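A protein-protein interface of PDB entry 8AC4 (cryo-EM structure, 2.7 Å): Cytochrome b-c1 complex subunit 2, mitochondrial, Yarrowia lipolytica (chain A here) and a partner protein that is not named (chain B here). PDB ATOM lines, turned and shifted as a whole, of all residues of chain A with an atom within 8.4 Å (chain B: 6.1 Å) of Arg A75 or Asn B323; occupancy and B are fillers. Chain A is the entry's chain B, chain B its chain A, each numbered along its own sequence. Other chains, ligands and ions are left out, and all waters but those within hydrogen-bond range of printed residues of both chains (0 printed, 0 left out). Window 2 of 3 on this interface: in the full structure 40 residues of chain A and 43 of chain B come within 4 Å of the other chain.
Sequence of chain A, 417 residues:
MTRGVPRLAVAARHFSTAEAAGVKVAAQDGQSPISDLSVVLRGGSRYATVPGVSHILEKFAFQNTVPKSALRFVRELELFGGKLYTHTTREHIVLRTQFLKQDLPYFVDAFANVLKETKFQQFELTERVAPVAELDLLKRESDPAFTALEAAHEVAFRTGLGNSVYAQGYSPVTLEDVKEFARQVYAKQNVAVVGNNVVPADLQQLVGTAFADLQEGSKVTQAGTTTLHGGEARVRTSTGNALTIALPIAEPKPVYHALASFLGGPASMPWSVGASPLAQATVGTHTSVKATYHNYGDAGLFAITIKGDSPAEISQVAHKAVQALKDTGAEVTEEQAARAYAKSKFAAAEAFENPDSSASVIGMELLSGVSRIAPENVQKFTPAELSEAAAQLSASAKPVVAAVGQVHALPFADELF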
ATOM      1  N   LYS A  68      38.952  -3.900   1.273  1.00  0.00           N
ATOM      2  CA  LYS A  68      37.630  -4.408   0.929  1.00  0.00           C
ATOM      3  C   LYS A  68      37.600  -4.786  -0.544  1.00  0.00           C
ATOM      4  O   LYS A  68      37.923  -3.959  -1.390  1.00  0.00           O
ATOM      5  CB  LYS A  68      36.583  -3.333   1.233  1.00  0.00           C
ATOM      6  CG  LYS A  68      35.126  -3.777   1.271  1.00  0.00           C
ATOM      7  CD  LYS A  68      34.157  -2.602   1.354  1.00  0.00           C
ATOM      8  CE  LYS A  68      34.007  -1.991   2.736  1.00  0.00           C
ATOM      9  NZ  LYS A  68      33.965  -3.003   3.820  1.00  0.00           N
ATOM     10  N   SER A  69      37.213  -6.034  -0.843  1.00  0.00           N
ATOM     11  CA  SER A  69      37.154  -6.501  -2.220  1.00  0.00           C
ATOM     12  C   SER A  69      35.961  -5.885  -2.932  1.00  0.00           C
ATOM     13  O   SER A  69      34.993  -5.470  -2.300  1.00  0.00           O
ATOM     14  CB  SER A  69      37.053  -7.990  -2.287  1.00  0.00           C
ATOM     15  OG  SER A  69      35.792  -8.411  -1.800  1.00  0.00           O
ATOM     16  N   ALA A  70      36.024  -5.887  -4.261  1.00  0.00           N
ATOM     17  CA  ALA A  70      34.909  -5.423  -5.066  1.00  0.00           C
ATOM     18  C   ALA A  70      33.645  -6.187  -4.684  1.00  0.00           C
ATOM     19  O   ALA A  70      32.595  -5.579  -4.518  1.00  0.00           O
ATOM     20  CB  ALA A  70      35.227  -5.599  -6.521  1.00  0.00           C
ATOM     21  N   LEU A  71      33.778  -7.509  -4.537  1.00  0.00           N
ATOM     22  CA  LEU A  71      32.672  -8.363  -4.154  1.00  0.00           C
ATOM     23  C   LEU A  71      32.117  -7.939  -2.798  1.00  0.00           C
ATOM     24  O   LEU A  71      30.917  -7.750  -2.670  1.00  0.00           O
ATOM     25  CB  LEU A  71      33.150  -9.810  -4.138  1.00  0.00           C
ATOM     26  CG  LEU A  71      32.210 -10.789  -3.451  1.00  0.00           C
ATOM     27  CD1 LEU A  71      30.897 -10.898  -4.210  1.00  0.00           C
ATOM     28  CD2 LEU A  71      32.874 -12.145  -3.339  1.00  0.00           C
ATOM     29  N   ARG A  72      32.972  -7.769  -1.792  1.00  0.00           N
ATOM     30  CA  ARG A  72      32.415  -7.411  -0.500  1.00  0.00           C
ATOM     31  C   ARG A  72      31.728  -6.049  -0.560  1.00  0.00           C
ATOM     32  O   ARG A  72      30.715  -5.831   0.091  1.00  0.00           O
ATOM     33  CB  ARG A  72      33.472  -7.375   0.596  1.00  0.00           C
ATOM     34  CG  ARG A  72      32.822  -7.090   1.938  1.00  0.00           C
ATOM     35  CD  ARG A  72      33.421  -7.688   3.194  1.00  0.00           C
ATOM     36  NE  ARG A  72      33.758  -9.109   3.163  1.00  0.00           N
ATOM     37  CZ  ARG A  72      33.268 -10.046   3.979  1.00  0.00           C
ATOM     38  NH1 ARG A  72      32.384  -9.734   4.913  1.00  0.00           N
ATOM     39  NH2 ARG A  72      33.669 -11.299   3.854  1.00  0.00           N
ATOM     40  N   PHE A  73      32.292  -5.117  -1.320  1.00  0.00           N
ATOM     41  CA  PHE A  73      31.680  -3.806  -1.411  1.00  0.00           C
ATOM     42  C   PHE A  73      30.287  -3.912  -2.028  1.00  0.00           C
ATOM     43  O   PHE A  73      29.337  -3.369  -1.483  1.00  0.00           O
ATOM     44  CB  PHE A  73      32.559  -2.845  -2.204  1.00  0.00           C
ATOM     45  CG  PHE A  73      31.891  -1.517  -2.435  1.00  0.00           C
ATOM     46  CD1 PHE A  73      31.724  -0.623  -1.382  1.00  0.00           C
ATOM     47  CD2 PHE A  73      31.384  -1.182  -3.683  1.00  0.00           C
ATOM     48  CE1 PHE A  73      31.071   0.587  -1.581  1.00  0.00           C
ATOM     49  CE2 PHE A  73      30.742   0.036  -3.884  1.00  0.00           C
ATOM     50  CZ  PHE A  73      30.584   0.917  -2.831  1.00  0.00           C
ATOM     51  N   VAL A  74      30.166  -4.612  -3.158  1.00  0.00           N
ATOM     52  CA  VAL A  74      28.874  -4.735  -3.813  1.00  0.00           C
ATOM     53  C   VAL A  74      27.855  -5.393  -2.884  1.00  0.00           C
ATOM     54  O   VAL A  74      26.713  -4.956  -2.835  1.00  0.00           O
ATOM     55  CB  VAL A  74      28.976  -5.484  -5.152  1.00  0.00           C
ATOM     56  CG1 VAL A  74      27.610  -5.873  -5.701  1.00  0.00           C
ATOM     57  CG2 VAL A  74      29.771  -4.697  -6.178  1.00  0.00           C
ATOM     58  N   ARG A  75      28.227  -6.469  -2.188  1.00  0.00           N
ATOM     59  CA  ARG A  75      27.247  -7.136  -1.345  1.00  0.00           C
ATOM     60  C   ARG A  75      26.841  -6.248  -0.174  1.00  0.00           C
ATOM     61  O   ARG A  75      25.732  -6.375   0.326  1.00  0.00           O
ATOM     62  CB  ARG A  75      27.761  -8.455  -0.771  1.00  0.00           C
ATOM     63  CG  ARG A  75      28.095  -9.517  -1.803  1.00  0.00           C
ATOM     64  CD  ARG A  75      26.878  -9.997  -2.550  1.00  0.00           C
ATOM     65  NE  ARG A  75      27.305 -10.983  -3.521  1.00  0.00           N
ATOM     66  CZ  ARG A  75      27.276 -12.293  -3.317  1.00  0.00           C
ATOM     67  NH1 ARG A  75      26.819 -12.775  -2.173  1.00  0.00           N
ATOM     68  NH2 ARG A  75      27.687 -13.117  -4.267  1.00  0.00           N
ATOM     69  N   GLU A  76      27.727  -5.365   0.283  1.00  0.00           N
ATOM     70  CA  GLU A  76      27.369  -4.555   1.435  1.00  0.00           C
ATOM     71  C   GLU A  76      26.564  -3.344   0.992  1.00  0.00           C
ATOM     72  O   GLU A  76      25.722  -2.847   1.732  1.00  0.00           O
ATOM     73  CB  GLU A  76      28.605  -4.092   2.187  1.00  0.00           C
ATOM     74  CG  GLU A  76      29.205  -5.172   3.053  1.00  0.00           C
ATOM     75  CD  GLU A  76      30.514  -4.749   3.696  1.00  0.00           C
ATOM     76  OE1 GLU A  76      30.951  -5.422   4.653  1.00  0.00           O
ATOM     77  OE2 GLU A  76      31.095  -3.737   3.247  1.00  0.00           O
ATOM     78  N   LEU A  77      26.848  -2.858  -0.212  1.00  0.00           N
ATOM     79  CA  LEU A  77      26.105  -1.748  -0.771  1.00  0.00           C
ATOM     80  C   LEU A  77      24.651  -2.170  -1.004  1.00  0.00           C
ATOM     81  O   LEU A  77      23.758  -1.342  -0.861  1.00  0.00           O
ATOM     82  CB  LEU A  77      26.834  -1.338  -2.052  1.00  0.00           C
ATOM     83  CG  LEU A  77      26.085  -0.439  -3.030  1.00  0.00           C
ATOM     84  CD1 LEU A  77      26.451   1.014  -2.789  1.00  0.00           C
ATOM     85  CD2 LEU A  77      26.429  -0.827  -4.459  1.00  0.00           C
ATOM     86  N   GLU A  78      24.421  -3.455  -1.318  1.00  0.00           N
ATOM     87  CA  GLU A  78      23.080  -4.010  -1.484  1.00  0.00           C
ATOM     88  C   GLU A  78      22.353  -4.110  -0.142  1.00  0.00           C
ATOM     89  O   GLU A  78      21.129  -4.082  -0.109  1.00  0.00           O
ATOM     90  CB  GLU A  78      23.098  -5.409  -2.108  1.00  0.00           C
ATOM     91  CG  GLU A  78      23.478  -5.444  -3.583  1.00  0.00           C
ATOM     92  CD  GLU A  78      23.344  -6.779  -4.310  1.00  0.00           C
ATOM     93  OE1 GLU A  78      22.770  -6.777  -5.419  1.00  0.00           O
ATOM     94  OE2 GLU A  78      23.798  -7.821  -3.780  1.00  0.00           O
ATOM     95  N   LEU A  79      23.084  -4.261   0.965  1.00  0.00           N
ATOM     96  CA  LEU A  79      22.454  -4.263   2.278  1.00  0.00           C
ATOM     97  C   LEU A  79      22.028  -2.866   2.716  1.00  0.00           C
ATOM     98  O   LEU A  79      21.245  -2.744   3.654  1.00  0.00           O
ATOM     99  CB  LEU A  79      23.460  -4.804   3.288  1.00  0.00           C
ATOM    100  CG  LEU A  79      23.283  -6.245   3.752  1.00  0.00           C
ATOM    101  CD1 LEU A  79      22.705  -7.150   2.672  1.00  0.00           C
ATOM    102  CD2 LEU A  79      24.615  -6.785   4.240  1.00  0.00           C
ATOM    103  N   PHE A  80      22.629  -1.826   2.136  1.00  0.00           N
ATOM    104  CA  PHE A  80      22.222  -0.469   2.452  1.00  0.00           C
ATOM    105  C   PHE A  80      21.273   0.043   1.377  1.00  0.00           C
ATOM    106  O   PHE A  80      20.783   1.173   1.445  1.00  0.00           O
ATOM    107  CB  PHE A  80      23.432   0.455   2.421  1.00  0.00           C
ATOM    108  CG  PHE A  80      24.264   0.479   3.673  1.00  0.00           C
ATOM    109  CD1 PHE A  80      23.693   0.605   4.932  1.00  0.00           C
ATOM    110  CD2 PHE A  80      25.640   0.348   3.587  1.00  0.00           C
ATOM    111  CE1 PHE A  80      24.489   0.625   6.070  1.00  0.00           C
ATOM    112  CE2 PHE A  80      26.432   0.367   4.726  1.00  0.00           C
ATOM    113  CZ  PHE A  80      25.860   0.519   5.966  1.00  0.00           C
ATOM    114  N   GLY A  81      21.085  -0.797   0.357  1.00  0.00           N
ATOM    115  CA  GLY A  81      20.310  -0.478  -0.827  1.00  0.00           C
ATOM    116  C   GLY A  81      20.832   0.747  -1.573  1.00  0.00           C
ATOM    117  O   GLY A  81      20.080   1.371  -2.315  1.00  0.00           O
ATOM    118  N   TYR A 106      29.735   5.159   6.027  1.00  0.00           N
ATOM    119  CA  TYR A 106      30.132   4.019   5.225  1.00  0.00           C
ATOM    120  C   TYR A 106      30.631   4.473   3.852  1.00  0.00           C
ATOM    121  O   TYR A 106      31.679   4.017   3.390  1.00  0.00           O
ATOM    122  CB  TYR A 106      28.990   3.000   5.132  1.00  0.00           C
ATOM    123  CG  TYR A 106      29.360   1.812   4.287  1.00  0.00           C
ATOM    124  CD1 TYR A 106      29.119   1.814   2.919  1.00  0.00           C
ATOM    125  CD2 TYR A 106      30.026   0.721   4.836  1.00  0.00           C
ATOM    126  CE1 TYR A 106      29.497   0.745   2.120  1.00  0.00           C
ATOM    127  CE2 TYR A 106      30.408  -0.357   4.052  1.00  0.00           C
ATOM    128  CZ  TYR A 106      30.140  -0.343   2.690  1.00  0.00           C
ATOM    129  OH  TYR A 106      30.515  -1.386   1.896  1.00  0.00           O
ATOM    130  N   ARG B 315      28.233  -8.509 -11.712  1.00  0.00           N
ATOM    131  CA  ARG B 315      28.803  -9.826 -11.502  1.00  0.00           C
ATOM    132  C   ARG B 315      28.945 -10.155 -10.014  1.00  0.00           C
ATOM    133  O   ARG B 315      29.193 -11.302  -9.660  1.00  0.00           O
ATOM    134  CB  ARG B 315      30.132  -9.936 -12.233  1.00  0.00           C
ATOM    135  CG  ARG B 315      31.273  -9.249 -11.508  1.00  0.00           C
ATOM    136  CD  ARG B 315      32.565  -9.700 -12.147  1.00  0.00           C
ATOM    137  NE  ARG B 315      32.712  -9.093 -13.462  1.00  0.00           N
ATOM    138  CZ  ARG B 315      32.811  -9.750 -14.615  1.00  0.00           C
ATOM    139  NH1 ARG B 315      32.831 -11.075 -14.654  1.00  0.00           N
ATOM    140  NH2 ARG B 315      32.932  -9.065 -15.740  1.00  0.00           N
ATOM    141  N   HIS B 316      28.774  -9.167  -9.136  1.00  0.00           N
ATOM    142  CA  HIS B 316      28.985  -9.412  -7.721  1.00  0.00           C
ATOM    143  C   HIS B 316      27.689  -9.407  -6.924  1.00  0.00           C
ATOM    144  O   HIS B 316      27.734  -9.498  -5.698  1.00  0.00           O
ATOM    145  CB  HIS B 316      29.930  -8.367  -7.152  1.00  0.00           C
ATOM    146  CG  HIS B 316      31.276  -8.465  -7.760  1.00  0.00           C
ATOM    147  ND1 HIS B 316      31.963  -9.665  -7.806  1.00  0.00           N
ATOM    148  CD2 HIS B 316      32.050  -7.542  -8.367  1.00  0.00           C
ATOM    149  CE1 HIS B 316      33.117  -9.472  -8.399  1.00  0.00           C
ATOM    150  NE2 HIS B 316      33.199  -8.174  -8.747  1.00  0.00           N
ATOM    151  N   GLN B 317      26.547  -9.289  -7.596  1.00  0.00           N
ATOM    152  CA  GLN B 317      25.269  -9.265  -6.897  1.00  0.00           C
ATOM    153  C   GLN B 317      25.018 -10.567  -6.136  1.00  0.00           C
ATOM    154  O   GLN B 317      25.484 -11.639  -6.516  1.00  0.00           O
ATOM    155  CB  GLN B 317      24.148  -9.057  -7.900  1.00  0.00           C
ATOM    156  CG  GLN B 317      24.215  -7.688  -8.535  1.00  0.00           C
ATOM    157  CD  GLN B 317      23.067  -7.452  -9.484  1.00  0.00           C
ATOM    158  OE1 GLN B 317      22.391  -6.426  -9.410  1.00  0.00           O
ATOM    159  NE2 GLN B 317      22.844  -8.389 -10.398  1.00  0.00           N
ATOM    160  N   GLY B 318      24.213 -10.469  -5.077  1.00  0.00           N
ATOM    161  CA  GLY B 318      23.974 -11.592  -4.186  1.00  0.00           C
ATOM    162  C   GLY B 318      22.973 -12.620  -4.710  1.00  0.00           C
ATOM    163  O   GLY B 318      23.034 -13.782  -4.306  1.00  0.00           O
ATOM    164  N   SER B 319      22.007 -12.158  -5.514  1.00  0.00           N
ATOM    165  CA  SER B 319      20.987 -12.967  -6.170  1.00  0.00           C
ATOM    166  C   SER B 319      21.570 -14.243  -6.776  1.00  0.00           C
ATOM    167  O   SER B 319      22.533 -14.191  -7.537  1.00  0.00           O
ATOM    168  CB  SER B 319      20.298 -12.143  -7.233  1.00  0.00           C
ATOM    169  OG  SER B 319      19.560 -12.961  -8.137  1.00  0.00           O
ATOM    170  N   ARG B 320      20.938 -15.382  -6.480  1.00  0.00           N
ATOM    171  CA  ARG B 320      21.417 -16.665  -6.961  1.00  0.00           C
ATOM    172  C   ARG B 320      21.319 -16.738  -8.485  1.00  0.00           C
ATOM    173  O   ARG B 320      22.239 -17.222  -9.148  1.00  0.00           O
ATOM    174  CB  ARG B 320      20.704 -17.803  -6.232  1.00  0.00           C
ATOM    175  CG  ARG B 320      21.017 -19.182  -6.787  1.00  0.00           C
ATOM    176  CD  ARG B 320      22.469 -19.576  -6.598  1.00  0.00           C
ATOM    177  NE  ARG B 320      22.754 -20.873  -7.201  1.00  0.00           N
ATOM    178  CZ  ARG B 320      23.967 -21.402  -7.355  1.00  0.00           C
ATOM    179  NH1 ARG B 320      25.045 -20.747  -6.954  1.00  0.00           N
ATOM    180  NH2 ARG B 320      24.099 -22.593  -7.917  1.00  0.00           N
ATOM    181  N   LEU B 321      20.226 -16.204  -9.042  1.00  0.00           N
ATOM    182  CA  LEU B 321      20.066 -16.254 -10.484  1.00  0.00           C
ATOM    183  C   LEU B 321      21.149 -15.416 -11.152  1.00  0.00           C
ATOM    184  O   LEU B 321      21.702 -15.808 -12.173  1.00  0.00           O
ATOM    185  CB  LEU B 321      18.675 -15.770 -10.896  1.00  0.00           C
ATOM    186  CG  LEU B 321      18.416 -15.870 -12.400  1.00  0.00           C
ATOM    187  CD1 LEU B 321      18.555 -17.297 -12.902  1.00  0.00           C
ATOM    188  CD2 LEU B 321      17.062 -15.311 -12.761  1.00  0.00           C
ATOM    189  N   SER B 322      21.455 -14.271 -10.549  1.00  0.00           N
ATOM    190  CA  SER B 322      22.487 -13.409 -11.075  1.00  0.00           C
ATOM    191  C   SER B 322      23.809 -14.171 -11.141  1.00  0.00           C
ATOM    192  O   SER B 322      24.508 -14.097 -12.149  1.00  0.00           O
ATOM    193  CB  SER B 322      22.603 -12.192 -10.235  1.00  0.00           C
ATOM    194  OG  SER B 322      23.575 -11.319 -10.780  1.00  0.00           O
ATOM    195  N   ASN B 323      24.124 -14.926 -10.085  1.00  0.00           N
ATOM    196  CA  ASN B 323      25.371 -15.668 -10.070  1.00  0.00           C
ATOM    197  C   ASN B 323      25.402 -16.718 -11.167  1.00  0.00           C
ATOM    198  O   ASN B 323      26.394 -16.814 -11.871  1.00  0.00           O
ATOM    199  CB  ASN B 323      25.690 -16.249  -8.699  1.00  0.00           C
ATOM    200  CG  ASN B 323      26.064 -15.136  -7.753  1.00  0.00           C
ATOM    201  OD1 ASN B 323      27.140 -14.560  -7.882  1.00  0.00           O
ATOM    202  ND2 ASN B 323      25.172 -14.791  -6.838  1.00  0.00           N
ATOM    203  N   ILE B 324      24.321 -17.486 -11.312  1.00  0.00           N
ATOM    204  CA  ILE B 324      24.296 -18.556 -12.296  1.00  0.00           C
ATOM    205  C   ILE B 324      24.474 -17.958 -13.687  1.00  0.00           C
ATOM    206  O   ILE B 324      25.186 -18.509 -14.520  1.00  0.00           O
ATOM    207  CB  ILE B 324      22.975 -19.342 -12.220  1.00  0.00           C
ATOM    208  CG1 ILE B 324      22.849 -20.153 -10.927  1.00  0.00           C
ATOM    209  CG2 ILE B 324      22.818 -20.221 -13.449  1.00  0.00           C
ATOM    210  CD1 ILE B 324      21.419 -20.375 -10.489  1.00  0.00           C
ATOM    211  N   VAL B 325      23.756 -16.866 -13.933  1.00  0.00           N
ATOM    212  CA  VAL B 325      23.686 -16.286 -15.259  1.00  0.00           C
ATOM    213  C   VAL B 325      25.039 -15.686 -15.611  1.00  0.00           C
ATOM    214  O   VAL B 325      25.507 -15.870 -16.725  1.00  0.00           O
ATOM    215  CB  VAL B 325      22.534 -15.272 -15.354  1.00  0.00           C
ATOM    216  CG1 VAL B 325      22.696 -14.305 -16.517  1.00  0.00           C
ATOM    217  CG2 VAL B 325      21.206 -15.999 -15.448  1.00  0.00           C
ATOM    218  N   SER B 326      25.661 -14.999 -14.651  1.00  0.00           N
ATOM    219  CA  SER B 326      26.911 -14.325 -14.946  1.00  0.00           C
ATOM    220  C   SER B 326      28.045 -15.328 -15.134  1.00  0.00           C
ATOM    221  O   SER B 326      28.800 -15.182 -16.088  1.00  0.00           O
ATOM    222  CB  SER B 326      27.238 -13.245 -13.959  1.00  0.00           C
ATOM    223  OG  SER B 326      27.436 -13.798 -12.671  1.00  0.00           O
ATOM    224  N   GLU B 327      28.111 -16.372 -14.289  1.00  0.00           N
ATOM    225  CA  GLU B 327      29.179 -17.367 -14.368  1.00  0.00           C
ATOM    226  C   GLU B 327      29.124 -18.141 -15.683  1.00  0.00           C
ATOM    227  O   GLU B 327      30.155 -18.532 -16.227  1.00  0.00           O
ATOM    228  CB  GLU B 327      29.134 -18.363 -13.209  1.00  0.00           C
ATOM    229  CG  GLU B 327      29.466 -17.742 -11.864  1.00  0.00           C
ATOM    230  CD  GLU B 327      29.255 -18.649 -10.661  1.00  0.00           C
ATOM    231  OE1 GLU B 327      28.099 -19.054 -10.404  1.00  0.00           O
ATOM    232  OE2 GLU B 327      30.257 -18.960  -9.986  1.00  0.00           O
ATOM    233  N   ASN B 328      27.915 -18.333 -16.205  1.00  0.00           N
ATOM    234  CA  ASN B 328      27.709 -19.203 -17.343  1.00  0.00           C
ATOM    235  C   ASN B 328      27.477 -18.427 -18.637  1.00  0.00           C
ATOM    236  O   ASN B 328      27.245 -19.048 -19.674  1.00  0.00           O
ATOM    237  CB  ASN B 328      26.608 -20.201 -17.012  1.00  0.00           C
ATOM    238  CG  ASN B 328      27.074 -21.149 -15.933  1.00  0.00           C
ATOM    239  OD1 ASN B 328      27.932 -21.991 -16.179  1.00  0.00           O
ATOM    240  ND2 ASN B 328      26.567 -20.985 -14.726  1.00  0.00           N
ATOM    241  N   ARG B 384      17.606  -9.616   3.369  1.00  0.00           N
ATOM    242  CA  ARG B 384      18.464  -8.935   2.416  1.00  0.00           C
ATOM    243  C   ARG B 384      17.621  -8.100   1.449  1.00  0.00           C
ATOM    244  O   ARG B 384      18.013  -6.992   1.105  1.00  0.00           O
ATOM    245  CB  ARG B 384      19.354  -9.941   1.674  1.00  0.00           C
ATOM    246  CG  ARG B 384      20.553 -10.465   2.458  1.00  0.00           C
ATOM    247  CD  ARG B 384      21.606 -11.171   1.610  1.00  0.00           C
ATOM    248  NE  ARG B 384      21.162 -12.437   1.035  1.00  0.00           N
ATOM    249  CZ  ARG B 384      21.107 -12.745  -0.266  1.00  0.00           C
ATOM    250  NH1 ARG B 384      20.664 -13.936  -0.630  1.00  0.00           N
ATOM    251  NH2 ARG B 384      21.500 -11.891  -1.202  1.00  0.00           N
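O of His B316 sits at hydrogen-bond distance from NE of Arg A75 (2.7 Å).
The backbone NH (N) of Gly B318 lies within hydrogen-bond range of the side-chain carboxylate (OE2) of Glu A78, at 3.0 Å.
The guanidinium group (NE) of Arg A75 lies close to the backbone NH (N) of Gly B318, 3.5 Å away.
O of Gln B317 lies within hydrogen-bond range of NH2 of Arg A75.
Ala A70 touches His B316 (CB to NE2, 3.96 Å).
Leu A71 touches His B316 (CD1 to O, 3.8 Å).
His B316 touches Val A74 (O to CG1, 3.6 Å).
Asn B323 touches Arg A75 (OD1 to NH2, 3.9 Å).
Glu A78 touches Gln B317 (OE1 to CG, 3.6 Å).
CD1 of Leu A79 touches CG of Arg B384, 3.96 Å away.
Of the 15 printed residues of chain B, 5 touch a printed residue of chain A.
Hydrophobic or aromatic side chains of chain B within 4 Å of the printed part of chain A: His B316.
Hydrophobic or aromatic side chains of chain A that line the printed part of chain B: Ala A70, Leu A71, Val A74 and Leu A79.
Among the printed residues, 10 pairs touch across the chains.
Among the printed residues, no Asp or Glu carboxylate lies within 4 Å of a Lys or Arg side-chain nitrogen of the other chain.
Of chain B, only His B316, Gln B317, Gly B318 and Asn B323 come within 4 Å of Arg A75.
Gly B318 touches two residues of chain A.
Of the printed residues of chain A, Gln B317 touches Arg A75 (3.5 Å) and Glu A78 (3.6 Å).
Of the printed residues of chain B, Leu A71 touches His B316.
Printed residues of chain B within 4 Å of Ala A70: His B316.
Of the printed residues of chain B, Glu A78 touches Gln B317 (3.6 Å) and Gly B318 (3.0 Å).
Printed residues of chain B within 4 Å of Leu A79: Arg B384 (3.96 Å).
Arg B315 touches none of the printed residues of chain A.
Gly A81 touches none of the printed residues of chain B.
The nearest residue of chain B that does not touch Arg A75 is Arg B384 (5.5 Å).
The nearest printed residue of chain B that does not touch Val A74 is Gln B317 (4.05 Å).
The side-chain amide nitrogen (NE2) of Gln B317 sits at hydrogen-bond distance from the side-chain hydroxyl (OG) of Ser B322.
OG of Ser B326 lies within hydrogen-bond range of O of Asn B323 (3.3 Å).
O of Gly B318 lies within hydrogen-bond range of ND2 of Asn B323 (3.5 Å).
The side-chain amide nitrogen (ND2) of Asn B323 lies within hydrogen-bond range of the backbone carbonyl oxygen (O) of Ser B319, at 2.8 Å.
O of Gln B317 is in hydrogen-bond range of ND2 of Asn B323 (3.2 Å).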
